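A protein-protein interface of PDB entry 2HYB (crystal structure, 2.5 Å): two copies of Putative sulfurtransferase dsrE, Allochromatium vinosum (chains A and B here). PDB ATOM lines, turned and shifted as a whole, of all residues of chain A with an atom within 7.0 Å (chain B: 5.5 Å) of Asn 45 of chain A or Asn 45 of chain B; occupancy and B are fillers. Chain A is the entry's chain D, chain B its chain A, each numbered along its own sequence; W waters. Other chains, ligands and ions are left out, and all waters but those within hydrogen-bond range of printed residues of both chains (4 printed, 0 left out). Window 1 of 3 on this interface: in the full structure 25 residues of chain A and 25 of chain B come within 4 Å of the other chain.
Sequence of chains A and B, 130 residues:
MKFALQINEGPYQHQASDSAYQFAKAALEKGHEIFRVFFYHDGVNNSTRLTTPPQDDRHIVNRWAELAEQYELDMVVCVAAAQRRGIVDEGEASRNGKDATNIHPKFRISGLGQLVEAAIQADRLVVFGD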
ATOM      1  N   GLU A   9      30.282   7.305 -27.573  1.00  0.00           N
ATOM      2  CA  GLU A   9      29.236   7.567 -28.546  1.00  0.00           C
ATOM      3  C   GLU A   9      27.945   6.805 -28.291  1.00  0.00           C
ATOM      4  O   GLU A   9      27.918   5.804 -27.578  1.00  0.00           O
ATOM      5  CB  GLU A   9      29.775   7.278 -29.942  1.00  0.00           C
ATOM      6  CG  GLU A   9      31.068   8.024 -30.262  1.00  0.00           C
ATOM      7  CD  GLU A   9      30.930   9.548 -30.194  1.00  0.00           C
ATOM      8  OE1 GLU A   9      29.870  10.096 -30.592  1.00  0.00           O
ATOM      9  OE2 GLU A   9      31.903  10.205 -29.763  1.00  0.00           O
ATOM     10  N   GLY A  10      26.864   7.312 -28.861  1.00  0.00           N
ATOM     11  CA  GLY A  10      25.577   6.676 -28.692  1.00  0.00           C
ATOM     12  C   GLY A  10      25.488   5.436 -29.553  1.00  0.00           C
ATOM     13  O   GLY A  10      26.357   5.201 -30.398  1.00  0.00           O
ATOM     14  N   PRO A  11      24.434   4.624 -29.373  1.00  0.00           N
ATOM     15  CA  PRO A  11      24.248   3.392 -30.148  1.00  0.00           C
ATOM     16  C   PRO A  11      23.827   3.599 -31.595  1.00  0.00           C
ATOM     17  O   PRO A  11      23.072   4.514 -31.898  1.00  0.00           O
ATOM     18  CB  PRO A  11      23.192   2.654 -29.341  1.00  0.00           C
ATOM     19  CG  PRO A  11      22.341   3.788 -28.812  1.00  0.00           C
ATOM     20  CD  PRO A  11      23.383   4.767 -28.345  1.00  0.00           C
ATOM     21  N   PHE A  39      30.115   5.153 -19.440  1.00  0.00           N
ATOM     22  CA  PHE A  39      29.598   5.830 -20.630  1.00  0.00           C
ATOM     23  C   PHE A  39      29.654   7.340 -20.456  1.00  0.00           C
ATOM     24  O   PHE A  39      29.183   7.880 -19.460  1.00  0.00           O
ATOM     25  CB  PHE A  39      28.149   5.409 -20.922  1.00  0.00           C
ATOM     26  CG  PHE A  39      27.991   3.955 -21.295  1.00  0.00           C
ATOM     27  CD1 PHE A  39      27.939   2.969 -20.311  1.00  0.00           C
ATOM     28  CD2 PHE A  39      27.888   3.569 -22.636  1.00  0.00           C
ATOM     29  CE1 PHE A  39      27.784   1.617 -20.662  1.00  0.00           C
ATOM     30  CE2 PHE A  39      27.734   2.224 -22.992  1.00  0.00           C
ATOM     31  CZ  PHE A  39      27.681   1.249 -22.006  1.00  0.00           C
ATOM     32  N   TYR A  40      30.227   8.023 -21.436  1.00  0.00           N
ATOM     33  CA  TYR A  40      30.354   9.478 -21.382  1.00  0.00           C
ATOM     34  C   TYR A  40      29.921  10.066 -22.718  1.00  0.00           C
ATOM     35  O   TYR A  40      29.862   9.353 -23.726  1.00  0.00           O
ATOM     36  CB  TYR A  40      31.805   9.856 -21.080  1.00  0.00           C
ATOM     37  CG  TYR A  40      32.041  11.289 -20.657  1.00  0.00           C
ATOM     38  CD1 TYR A  40      31.280  11.873 -19.650  1.00  0.00           C
ATOM     39  CD2 TYR A  40      33.086  12.038 -21.211  1.00  0.00           C
ATOM     40  CE1 TYR A  40      31.551  13.156 -19.194  1.00  0.00           C
ATOM     41  CE2 TYR A  40      33.363  13.328 -20.761  1.00  0.00           C
ATOM     42  CZ  TYR A  40      32.593  13.877 -19.748  1.00  0.00           C
ATOM     43  OH  TYR A  40      32.878  15.130 -19.264  1.00  0.00           O
ATOM     44  N   HIS A  41      29.630  11.363 -22.725  1.00  0.00           N
ATOM     45  CA  HIS A  41      29.175  12.055 -23.928  1.00  0.00           C
ATOM     46  C   HIS A  41      27.867  11.401 -24.355  1.00  0.00           C
ATOM     47  O   HIS A  41      27.042  11.074 -23.512  1.00  0.00           O
ATOM     48  CB  HIS A  41      30.201  11.941 -25.064  1.00  0.00           C
ATOM     49  CG  HIS A  41      31.551  12.484 -24.720  1.00  0.00           C
ATOM     50  ND1 HIS A  41      31.754  13.792 -24.332  1.00  0.00           N
ATOM     51  CD2 HIS A  41      32.774  11.898 -24.714  1.00  0.00           C
ATOM     52  CE1 HIS A  41      33.040  13.988 -24.106  1.00  0.00           C
ATOM     53  NE2 HIS A  41      33.681  12.854 -24.330  1.00  0.00           N
ATOM     54  N   ASP A  42      27.684  11.218 -25.657  1.00  0.00           N
ATOM     55  CA  ASP A  42      26.495  10.572 -26.200  1.00  0.00           C
ATOM     56  C   ASP A  42      26.506   9.116 -25.788  1.00  0.00           C
ATOM     57  O   ASP A  42      25.525   8.413 -25.970  1.00  0.00           O
ATOM     58  CB  ASP A  42      26.488  10.633 -27.725  1.00  0.00           C
ATOM     59  CG  ASP A  42      25.819  11.875 -28.253  1.00  0.00           C
ATOM     60  OD1 ASP A  42      25.397  12.723 -27.436  1.00  0.00           O
ATOM     61  OD2 ASP A  42      25.708  12.000 -29.489  1.00  0.00           O
ATOM     62  N   GLY A  43      27.629   8.660 -25.255  1.00  0.00           N
ATOM     63  CA  GLY A  43      27.716   7.288 -24.811  1.00  0.00           C
ATOM     64  C   GLY A  43      26.573   6.967 -23.865  1.00  0.00           C
ATOM     65  O   GLY A  43      25.996   5.887 -23.950  1.00  0.00           O
ATOM     66  N   VAL A  44      26.227   7.895 -22.974  1.00  0.00           N
ATOM     67  CA  VAL A  44      25.148   7.645 -22.032  1.00  0.00           C
ATOM     68  C   VAL A  44      23.888   7.127 -22.709  1.00  0.00           C
ATOM     69  O   VAL A  44      23.058   6.485 -22.069  1.00  0.00           O
ATOM     70  CB  VAL A  44      24.738   8.906 -21.245  1.00  0.00           C
ATOM     71  CG1 VAL A  44      25.873   9.376 -20.354  1.00  0.00           C
ATOM     72  CG2 VAL A  44      24.289   9.993 -22.202  1.00  0.00           C
ATOM     73  N   ASN A  45      23.725   7.398 -23.996  1.00  0.00           N
ATOM     74  CA  ASN A  45      22.526   6.936 -24.683  1.00  0.00           C
ATOM     75  C   ASN A  45      22.457   5.435 -24.893  1.00  0.00           C
ATOM     76  O   ASN A  45      21.549   4.928 -25.549  1.00  0.00           O
ATOM     77  CB  ASN A  45      22.372   7.679 -26.003  1.00  0.00           C
ATOM     78  CG  ASN A  45      21.963   9.120 -25.792  1.00  0.00           C
ATOM     79  OD1 ASN A  45      22.008   9.946 -26.711  1.00  0.00           O
ATOM     80  ND2 ASN A  45      21.551   9.432 -24.567  1.00  0.00           N
ATOM     81  N   ASN A  46      23.412   4.718 -24.328  1.00  0.00           N
ATOM     82  CA  ASN A  46      23.422   3.267 -24.438  1.00  0.00           C
ATOM     83  C   ASN A  46      22.739   2.692 -23.193  1.00  0.00           C
ATOM     84  O   ASN A  46      22.786   1.495 -22.935  1.00  0.00           O
ATOM     85  CB  ASN A  46      24.866   2.758 -24.535  1.00  0.00           C
ATOM     86  CG  ASN A  46      25.479   2.994 -25.906  1.00  0.00           C
ATOM     87  OD1 ASN A  46      25.150   2.306 -26.874  1.00  0.00           O
ATOM     88  ND2 ASN A  46      26.366   3.983 -25.999  1.00  0.00           N
ATOM     89  N   SER A  47      22.081   3.553 -22.427  1.00  0.00           N
ATOM     90  CA  SER A  47      21.438   3.087 -21.209  1.00  0.00           C
ATOM     91  C   SER A  47      19.922   3.246 -21.179  1.00  0.00           C
ATOM     92  O   SER A  47      19.295   2.977 -20.161  1.00  0.00           O
ATOM     93  CB  SER A  47      22.064   3.782 -19.986  1.00  0.00           C
ATOM     94  OG  SER A  47      21.819   5.177 -20.006  1.00  0.00           O
ATOM     95  N   THR A  48      19.323   3.692 -22.271  1.00  0.00           N
ATOM     96  CA  THR A  48      17.871   3.833 -22.255  1.00  0.00           C
ATOM     97  C   THR A  48      17.200   2.483 -22.515  1.00  0.00           C
ATOM     98  O   THR A  48      17.747   1.620 -23.215  1.00  0.00           O
ATOM     99  CB  THR A  48      17.370   4.881 -23.288  1.00  0.00           C
ATOM    100  OG1 THR A  48      15.937   4.921 -23.267  1.00  0.00           O
ATOM    101  CG2 THR A  48      17.835   4.529 -24.681  1.00  0.00           C
ATOM    102  N   THR A  51      14.401   1.735 -26.465  1.00  0.00           N
ATOM    103  CA  THR A  51      14.668   1.450 -27.866  1.00  0.00           C
ATOM    104  C   THR A  51      13.911   0.208 -28.339  1.00  0.00           C
ATOM    105  O   THR A  51      13.664  -0.713 -27.567  1.00  0.00           O
ATOM    106  CB  THR A  51      16.192   1.262 -28.150  1.00  0.00           C
ATOM    107  OG1 THR A  51      16.652   0.006 -27.630  1.00  0.00           O
ATOM    108  CG2 THR A  51      16.986   2.394 -27.528  1.00  0.00           C
ATOM    109  N   VAL A  61      21.347  -2.164 -26.585  1.00  0.00           N
ATOM    110  CA  VAL A  61      21.061  -2.006 -25.157  1.00  0.00           C
ATOM    111  C   VAL A  61      20.887  -3.345 -24.443  1.00  0.00           C
ATOM    112  O   VAL A  61      21.550  -3.607 -23.441  1.00  0.00           O
ATOM    113  CB  VAL A  61      19.797  -1.164 -24.891  1.00  0.00           C
ATOM    114  CG1 VAL A  61      19.635  -0.972 -23.388  1.00  0.00           C
ATOM    115  CG2 VAL A  61      19.896   0.185 -25.588  1.00  0.00           C
ATOM    116  N   VAL A  77      26.778   5.392 -15.989  1.00  0.00           N
ATOM    117  CA  VAL A  77      26.369   6.469 -16.900  1.00  0.00           C
ATOM    118  C   VAL A  77      26.672   7.812 -16.222  1.00  0.00           C
ATOM    119  O   VAL A  77      26.186   8.059 -15.118  1.00  0.00           O
ATOM    120  CB  VAL A  77      24.840   6.386 -17.183  1.00  0.00           C
ATOM    121  CG1 VAL A  77      24.387   7.566 -18.011  1.00  0.00           C
ATOM    122  CG2 VAL A  77      24.512   5.063 -17.885  1.00  0.00           C
ATOM    123  N   ALA A  81      26.332  14.127 -18.147  1.00  0.00           N
ATOM    124  CA  ALA A  81      26.117  13.814 -19.550  1.00  0.00           C
ATOM    125  C   ALA A  81      24.675  13.344 -19.751  1.00  0.00           C
ATOM    126  O   ALA A  81      24.040  13.664 -20.756  1.00  0.00           O
ATOM    127  CB  ALA A  81      27.112  12.738 -20.006  1.00  0.00           C
ATOM    128  N   ALA A  82      24.160  12.596 -18.781  1.00  0.00           N
ATOM    129  CA  ALA A  82      22.794  12.077 -18.848  1.00  0.00           C
ATOM    130  C   ALA A  82      21.765  13.198 -18.733  1.00  0.00           C
ATOM    131  O   ALA A  82      20.732  13.180 -19.394  1.00  0.00           O
ATOM    132  CB  ALA A  82      22.577  11.041 -17.748  1.00  0.00           C
ATOM    133  N   ARG A  84      22.154  16.360 -19.645  1.00  0.00           N
ATOM    134  CA  ARG A  84      22.200  17.138 -20.886  1.00  0.00           C
ATOM    135  C   ARG A  84      21.502  16.438 -22.071  1.00  0.00           C
ATOM    136  O   ARG A  84      20.953  17.095 -22.967  1.00  0.00           O
ATOM    137  CB  ARG A  84      23.672  17.403 -21.258  1.00  0.00           C
ATOM    138  CG  ARG A  84      23.945  18.763 -21.892  1.00  0.00           C
ATOM    139  CD  ARG A  84      25.434  19.028 -22.112  1.00  0.00           C
ATOM    140  NE  ARG A  84      26.239  18.663 -20.953  1.00  0.00           N
ATOM    141  CZ  ARG A  84      27.375  19.263 -20.603  1.00  0.00           C
ATOM    142  NH1 ARG A  84      27.848  20.275 -21.321  1.00  0.00           N
ATOM    143  NH2 ARG A  84      28.047  18.841 -19.535  1.00  0.00           N
ATOM    144  N   ARG A  85      21.515  15.107 -22.056  1.00  0.00           N
ATOM    145  CA  ARG A  85      20.950  14.333 -23.148  1.00  0.00           C
ATOM    146  C   ARG A  85      19.607  13.660 -22.884  1.00  0.00           C
ATOM    147  O   ARG A  85      18.924  13.262 -23.825  1.00  0.00           O
ATOM    148  CB  ARG A  85      21.990  13.313 -23.596  1.00  0.00           C
ATOM    149  CG  ARG A  85      23.274  13.966 -24.082  1.00  0.00           C
ATOM    150  CD  ARG A  85      24.377  12.948 -24.312  1.00  0.00           C
ATOM    151  NE  ARG A  85      25.578  13.512 -24.932  1.00  0.00           N
ATOM    152  CZ  ARG A  85      26.448  14.315 -24.324  1.00  0.00           C
ATOM    153  NH1 ARG A  85      26.264  14.670 -23.063  1.00  0.00           N
ATOM    154  NH2 ARG A  85      27.521  14.748 -24.974  1.00  0.00           N
ATOM    155  N   GLY A  86      19.230  13.527 -21.614  1.00  0.00           N
ATOM    156  CA  GLY A  86      17.950  12.926 -21.297  1.00  0.00           C
ATOM    157  C   GLY A  86      17.906  11.525 -20.706  1.00  0.00           C
ATOM    158  O   GLY A  86      16.896  10.839 -20.853  1.00  0.00           O
ATOM    159  N   ILE A  87      18.973  11.064 -20.063  1.00  0.00           N
ATOM    160  CA  ILE A  87      18.921   9.745 -19.448  1.00  0.00           C
ATOM    161  C   ILE A  87      18.475   9.954 -18.010  1.00  0.00           C
ATOM    162  O   ILE A  87      19.183  10.565 -17.219  1.00  0.00           O
ATOM    163  CB  ILE A  87      20.276   9.046 -19.489  1.00  0.00           C
ATOM    164  CG1 ILE A  87      20.613   8.678 -20.936  1.00  0.00           C
ATOM    165  CG2 ILE A  87      20.253   7.799 -18.617  1.00  0.00           C
ATOM    166  CD1 ILE A  87      19.699   7.618 -21.552  1.00  0.00           C
ATOM    167  N   ASN A 102      13.650   6.581 -18.082  1.00  0.00           N
ATOM    168  CA  ASN A 102      13.899   5.783 -19.263  1.00  0.00           C
ATOM    169  C   ASN A 102      15.154   4.936 -19.145  1.00  0.00           C
ATOM    170  O   ASN A 102      15.465   4.160 -20.052  1.00  0.00           O
ATOM    171  CB  ASN A 102      13.997   6.691 -20.498  1.00  0.00           C
ATOM    172  CG  ASN A 102      15.209   7.606 -20.461  1.00  0.00           C
ATOM    173  OD1 ASN A 102      15.727   7.928 -19.392  1.00  0.00           O
ATOM    174  ND2 ASN A 102      15.657   8.040 -21.630  1.00  0.00           N
ATOM    175  N   GLY B  10      22.533  14.797 -32.735  1.00  0.00           N
ATOM    176  CA  GLY B  10      21.924  15.053 -31.447  1.00  0.00           C
ATOM    177  C   GLY B  10      22.320  16.391 -30.849  1.00  0.00           C
ATOM    178  O   GLY B  10      23.243  17.060 -31.327  1.00  0.00           O
ATOM    179  N   PRO B  11      21.624  16.820 -29.794  1.00  0.00           N
ATOM    180  CA  PRO B  11      21.948  18.098 -29.162  1.00  0.00           C
ATOM    181  C   PRO B  11      23.314  18.078 -28.473  1.00  0.00           C
ATOM    182  O   PRO B  11      23.818  17.019 -28.112  1.00  0.00           O
ATOM    183  CB  PRO B  11      20.803  18.280 -28.177  1.00  0.00           C
ATOM    184  CG  PRO B  11      20.442  16.855 -27.819  1.00  0.00           C
ATOM    185  CD  PRO B  11      20.455  16.189 -29.157  1.00  0.00           C
ATOM    186  N   HIS B  41      18.586  10.438 -38.125  1.00  0.00           N
ATOM    187  CA  HIS B  41      19.772   9.957 -37.400  1.00  0.00           C
ATOM    188  C   HIS B  41      19.690  10.446 -35.948  1.00  0.00           C
ATOM    189  O   HIS B  41      18.599  10.682 -35.422  1.00  0.00           O
ATOM    190  CB  HIS B  41      21.064  10.517 -38.004  1.00  0.00           C
ATOM    191  CG  HIS B  41      21.225  10.267 -39.472  1.00  0.00           C
ATOM    192  ND1 HIS B  41      21.457   9.016 -39.999  1.00  0.00           N
ATOM    193  CD2 HIS B  41      21.213  11.121 -40.523  1.00  0.00           C
ATOM    194  CE1 HIS B  41      21.581   9.109 -41.312  1.00  0.00           C
ATOM    195  NE2 HIS B  41      21.438  10.377 -41.654  1.00  0.00           N
ATOM    196  N   ASP B  42      20.848  10.606 -35.306  1.00  0.00           N
ATOM    197  CA  ASP B  42      20.901  11.100 -33.932  1.00  0.00           C
ATOM    198  C   ASP B  42      20.108  12.411 -33.804  1.00  0.00           C
ATOM    199  O   ASP B  42      19.827  12.876 -32.698  1.00  0.00           O
ATOM    200  CB  ASP B  42      22.353  11.320 -33.487  1.00  0.00           C
ATOM    201  CG  ASP B  42      22.954  10.085 -32.829  1.00  0.00           C
ATOM    202  OD1 ASP B  42      22.219   9.088 -32.664  1.00  0.00           O
ATOM    203  OD2 ASP B  42      24.155  10.108 -32.473  1.00  0.00           O
ATOM    204  N   GLY B  43      19.738  13.004 -34.933  1.00  0.00           N
ATOM    205  CA  GLY B  43      18.952  14.225 -34.880  1.00  0.00           C
ATOM    206  C   GLY B  43      17.651  14.050 -34.090  1.00  0.00           C
ATOM    207  O   GLY B  43      17.220  14.963 -33.380  1.00  0.00           O
ATOM    208  N   VAL B  44      17.021  12.882 -34.196  1.00  0.00           N
ATOM    209  CA  VAL B  44      15.783  12.625 -33.479  1.00  0.00           C
ATOM    210  C   VAL B  44      15.892  12.861 -31.976  1.00  0.00           C
ATOM    211  O   VAL B  44      14.881  12.952 -31.289  1.00  0.00           O
ATOM    212  CB  VAL B  44      15.302  11.165 -33.690  1.00  0.00           C
ATOM    213  CG1 VAL B  44      14.994  10.921 -35.165  1.00  0.00           C
ATOM    214  CG2 VAL B  44      16.358  10.188 -33.174  1.00  0.00           C
ATOM    215  N   ASN B  45      17.104  12.948 -31.452  1.00  0.00           N
ATOM    216  CA  ASN B  45      17.261  13.141 -30.022  1.00  0.00           C
ATOM    217  C   ASN B  45      17.064  14.575 -29.564  1.00  0.00           C
ATOM    218  O   ASN B  45      17.148  14.868 -28.373  1.00  0.00           O
ATOM    219  CB  ASN B  45      18.618  12.614 -29.574  1.00  0.00           C
ATOM    220  CG  ASN B  45      18.668  11.102 -29.575  1.00  0.00           C
ATOM    221  OD1 ASN B  45      19.714  10.502 -29.366  1.00  0.00           O
ATOM    222  ND2 ASN B  45      17.522  10.476 -29.801  1.00  0.00           N
ATOM    223  N   ASN B  46      16.793  15.472 -30.501  1.00  0.00           N
ATOM    224  CA  ASN B  46      16.550  16.863 -30.139  1.00  0.00           C
ATOM    225  C   ASN B  46      15.082  16.977 -29.695  1.00  0.00           C
ATOM    226  O   ASN B  46      14.619  18.055 -29.308  1.00  0.00           O
ATOM    227  CB  ASN B  46      16.815  17.792 -31.347  1.00  0.00           C
ATOM    228  CG  ASN B  46      18.309  18.088 -31.566  1.00  0.00           C
ATOM    229  OD1 ASN B  46      18.906  18.883 -30.846  1.00  0.00           O
ATOM    230  ND2 ASN B  46      18.910  17.438 -32.555  1.00  0.00           N
ATOM    231  N   SER B  47      14.358  15.857 -29.728  1.00  0.00           N
ATOM    232  CA  SER B  47      12.942  15.868 -29.380  1.00  0.00           C
ATOM    233  C   SER B  47      12.537  15.338 -28.003  1.00  0.00           C
ATOM    234  O   SER B  47      11.356  15.366 -27.661  1.00  0.00           O
ATOM    235  CB  SER B  47      12.154  15.105 -30.439  1.00  0.00           C
ATOM    236  OG  SER B  47      12.342  13.708 -30.286  1.00  0.00           O
ATOM    237  N   THR B  48      13.483  14.848 -27.211  1.00  0.00           N
ATOM    238  CA  THR B  48      13.117  14.334 -25.891  1.00  0.00           C
ATOM    239  C   THR B  48      12.834  15.461 -24.897  1.00  0.00           C
ATOM    240  O   THR B  48      13.479  16.522 -24.931  1.00  0.00           O
ATOM    241  CB  THR B  48      14.218  13.383 -25.319  1.00  0.00           C
ATOM    242  OG1 THR B  48      13.931  13.076 -23.944  1.00  0.00           O
ATOM    243  CG2 THR B  48      15.599  14.030 -25.430  1.00  0.00           C
ATOM    244  N   VAL B  61      16.486  21.753 -26.518  1.00  0.00           N
ATOM    245  CA  VAL B  61      15.157  21.234 -26.787  1.00  0.00           C
ATOM    246  C   VAL B  61      14.064  22.276 -26.609  1.00  0.00           C
ATOM    247  O   VAL B  61      13.238  22.456 -27.499  1.00  0.00           O
ATOM    248  CB  VAL B  61      14.841  20.027 -25.904  1.00  0.00           C
ATOM    249  CG1 VAL B  61      13.472  19.473 -26.267  1.00  0.00           C
ATOM    250  CG2 VAL B  61      15.907  18.960 -26.087  1.00  0.00           C
ATOM    251  N   ARG B  85      16.993   4.675 -31.535  1.00  0.00           N
ATOM    252  CA  ARG B  85      17.644   5.442 -30.481  1.00  0.00           C
ATOM    253  C   ARG B  85      16.886   5.611 -29.175  1.00  0.00           C
ATOM    254  O   ARG B  85      17.503   5.861 -28.137  1.00  0.00           O
ATOM    255  CB  ARG B  85      18.041   6.802 -31.043  1.00  0.00           C
ATOM    256  CG  ARG B  85      18.979   6.660 -32.220  1.00  0.00           C
ATOM    257  CD  ARG B  85      19.142   7.938 -33.000  1.00  0.00           C
ATOM    258  NE  ARG B  85      20.116   7.739 -34.073  1.00  0.00           N
ATOM    259  CZ  ARG B  85      19.877   7.098 -35.216  1.00  0.00           C
ATOM    260  NH1 ARG B  85      18.680   6.589 -35.461  1.00  0.00           N
ATOM    261  NH2 ARG B  85      20.846   6.950 -36.110  1.00  0.00           N
ATOM    262  N   GLY B  86      15.561   5.484 -29.207  1.00  0.00           N
ATOM    263  CA  GLY B  86      14.812   5.611 -27.968  1.00  0.00           C
ATOM    264  C   GLY B  86      13.861   6.779 -27.785  1.00  0.00           C
ATOM    265  O   GLY B  86      13.575   7.160 -26.648  1.00  0.00           O
ATOM    266  N   ILE B  87      13.370   7.358 -28.878  1.00  0.00           N
ATOM    267  CA  ILE B  87      12.414   8.459 -28.772  1.00  0.00           C
ATOM    268  C   ILE B  87      11.027   7.830 -28.895  1.00  0.00           C
ATOM    269  O   ILE B  87      10.729   7.166 -29.895  1.00  0.00           O
ATOM    270  CB  ILE B  87      12.625   9.492 -29.875  1.00  0.00           C
ATOM    271  CG1 ILE B  87      14.005  10.134 -29.717  1.00  0.00           C
ATOM    272  CG2 ILE B  87      11.538  10.552 -29.802  1.00  0.00           C
ATOM    273  CD1 ILE B  87      14.177  10.910 -28.428  1.00  0.00           C
HETATM  274  O   HOH W   1      15.376  10.889 -23.394  1.00  0.00           O
HETATM  275  O   HOH W   2      26.357   9.822 -30.979  1.00  0.00           O
HETATM  276  O   HOH W   3      23.025  14.223 -28.165  1.00  0.00           O
HETATM  277  O   HOH W   4      15.200   7.180 -24.195  1.00  0.00           O
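The backbone NH (N) of Gly 10 of chain B lies close to the backbone carbonyl oxygen (O) of Asp 42 of chain B (3.3 Å).
NE of Arg 85 of chain B lies within salt-bridge range of OD1 of Asp 42 of chain B (2.9 Å).
The backbone NH of Gly 10 of chain A sits close to the backbone carbonyl oxygen of Asp 42 of chain A (3.4 Å).
The guanidinium group of Arg 85 of chain A sits close to the backbone carbonyl oxygen of His 41 of chain A (3.2 Å).
The side-chain hydroxyl (OG1) of Thr 48 of chain A lies close to the backbone carbonyl oxygen (O) of Asn 102 of chain A.
O of Ala 81 of chain A sits at hydrogen-bond distance from NH1 of Arg 85 of chain A (3.4 Å).
Val 44 of chain A touches none of the printed residues of chain B.
Asn 45 of chain A touches one residue of chain B.
Printed residues of chain B within 4 Å of Thr 48 of chain A: Arg 85 (3.7 Å).
Ala 81 of chain A touches none of the printed residues of chain B.
Of the printed residues of chain B, Arg 85 of chain A touches Thr 48 (3.8 Å).
Of the printed residues of chain A, Asp 42 of chain B touches Asp 42 (3.9 Å).
Asn 45 of chain B touches one residue of chain A.
Of the printed residues of chain A, Arg 85 of chain B touches Thr 48 (3.7 Å) and Thr 51 (3.6 Å).
The nearest residue of chain B that does not touch Asn 45 of chain A is Arg 85 of chain B (4.9 Å).
The nearest printed residue of chain B that does not touch Arg 85 of chain A is Pro 11 of chain B (5.1 Å).
Asp 42 of chain A touches its own counterpart, Asp 42 of chain B.
Asn 45 of chain B touches its own counterpart, Asn 45 of chain A.
Thr 48 of chain A touches Arg 85 of chain B, and with the chains exchanged Arg 85 of chain A touches Thr 48 of chain B.
Positions printed for both chains: 10, 11, 41, 42, 43, 44, 45, 46, 47, 48, 61, 85, 86 and 87.
Of the 6 pairs that touch across the chains among the printed residues, 4 have their exchanged pair printed and touching as well.
Water W4 lies within hydrogen-bond range of the side-chain hydroxyl (OG1) of Thr 48 of chain A (2.6 Å), the side-chain amide nitrogen (ND2) of Asn 102 of chain A (2.7 Å) and the backbone carbonyl oxygen (O) of Gly 86 of chain B (2.9 Å).
Water W2 lies within hydrogen-bond range of the side-chain carboxylate (OD2) of Asp 42 of chain B (2.7 Å), the side-chain carboxylate (OD2) of Asp 42 of chain A (2.7 Å) and the backbone NH (N) of Gly 10 of chain A (3.3 Å).
Water W1 lies within hydrogen-bond range of OG1 of Thr 48 of chain B (2.7 Å), O of Gly 86 of chain A (3.0 Å) and ND2 of Asn 102 of chain A (3.4 Å).
Water W3 bridges the side-chain carboxylate (OD1) of Asp 42 of chain A (2.9 Å) and the backbone carbonyl oxygen (O) of Pro 11 of chain B (2.9 Å).
Of the 14 printed residues of chain B, 5 touch a printed residue of chain A.
Of the 23 printed residues of chain A, 5 touch a printed residue of chain B.
Among the printed residues, 6 pairs touch across the chains.
Among the printed residues, no Asp or Glu carboxylate lies within 4 Å of a Lys or Arg side-chain nitrogen of the other chain.
Among the printed residues, pairs that only touch across the chains: Asn 45 of chain A with Asn 45 of chain B (3.6 Å), Thr 51 of chain A with Arg 85 of chain B (3.6 Å), Thr 48 of chain A with Arg 85 of chain B (3.7 Å), Arg 85 of chain A with Thr 48 of chain B (3.8 Å), Thr 51 of chain A with Gly 86 of chain B (3.8 Å) and Asp 42 of chain A with Asp 42 of chain B (3.9 Å).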
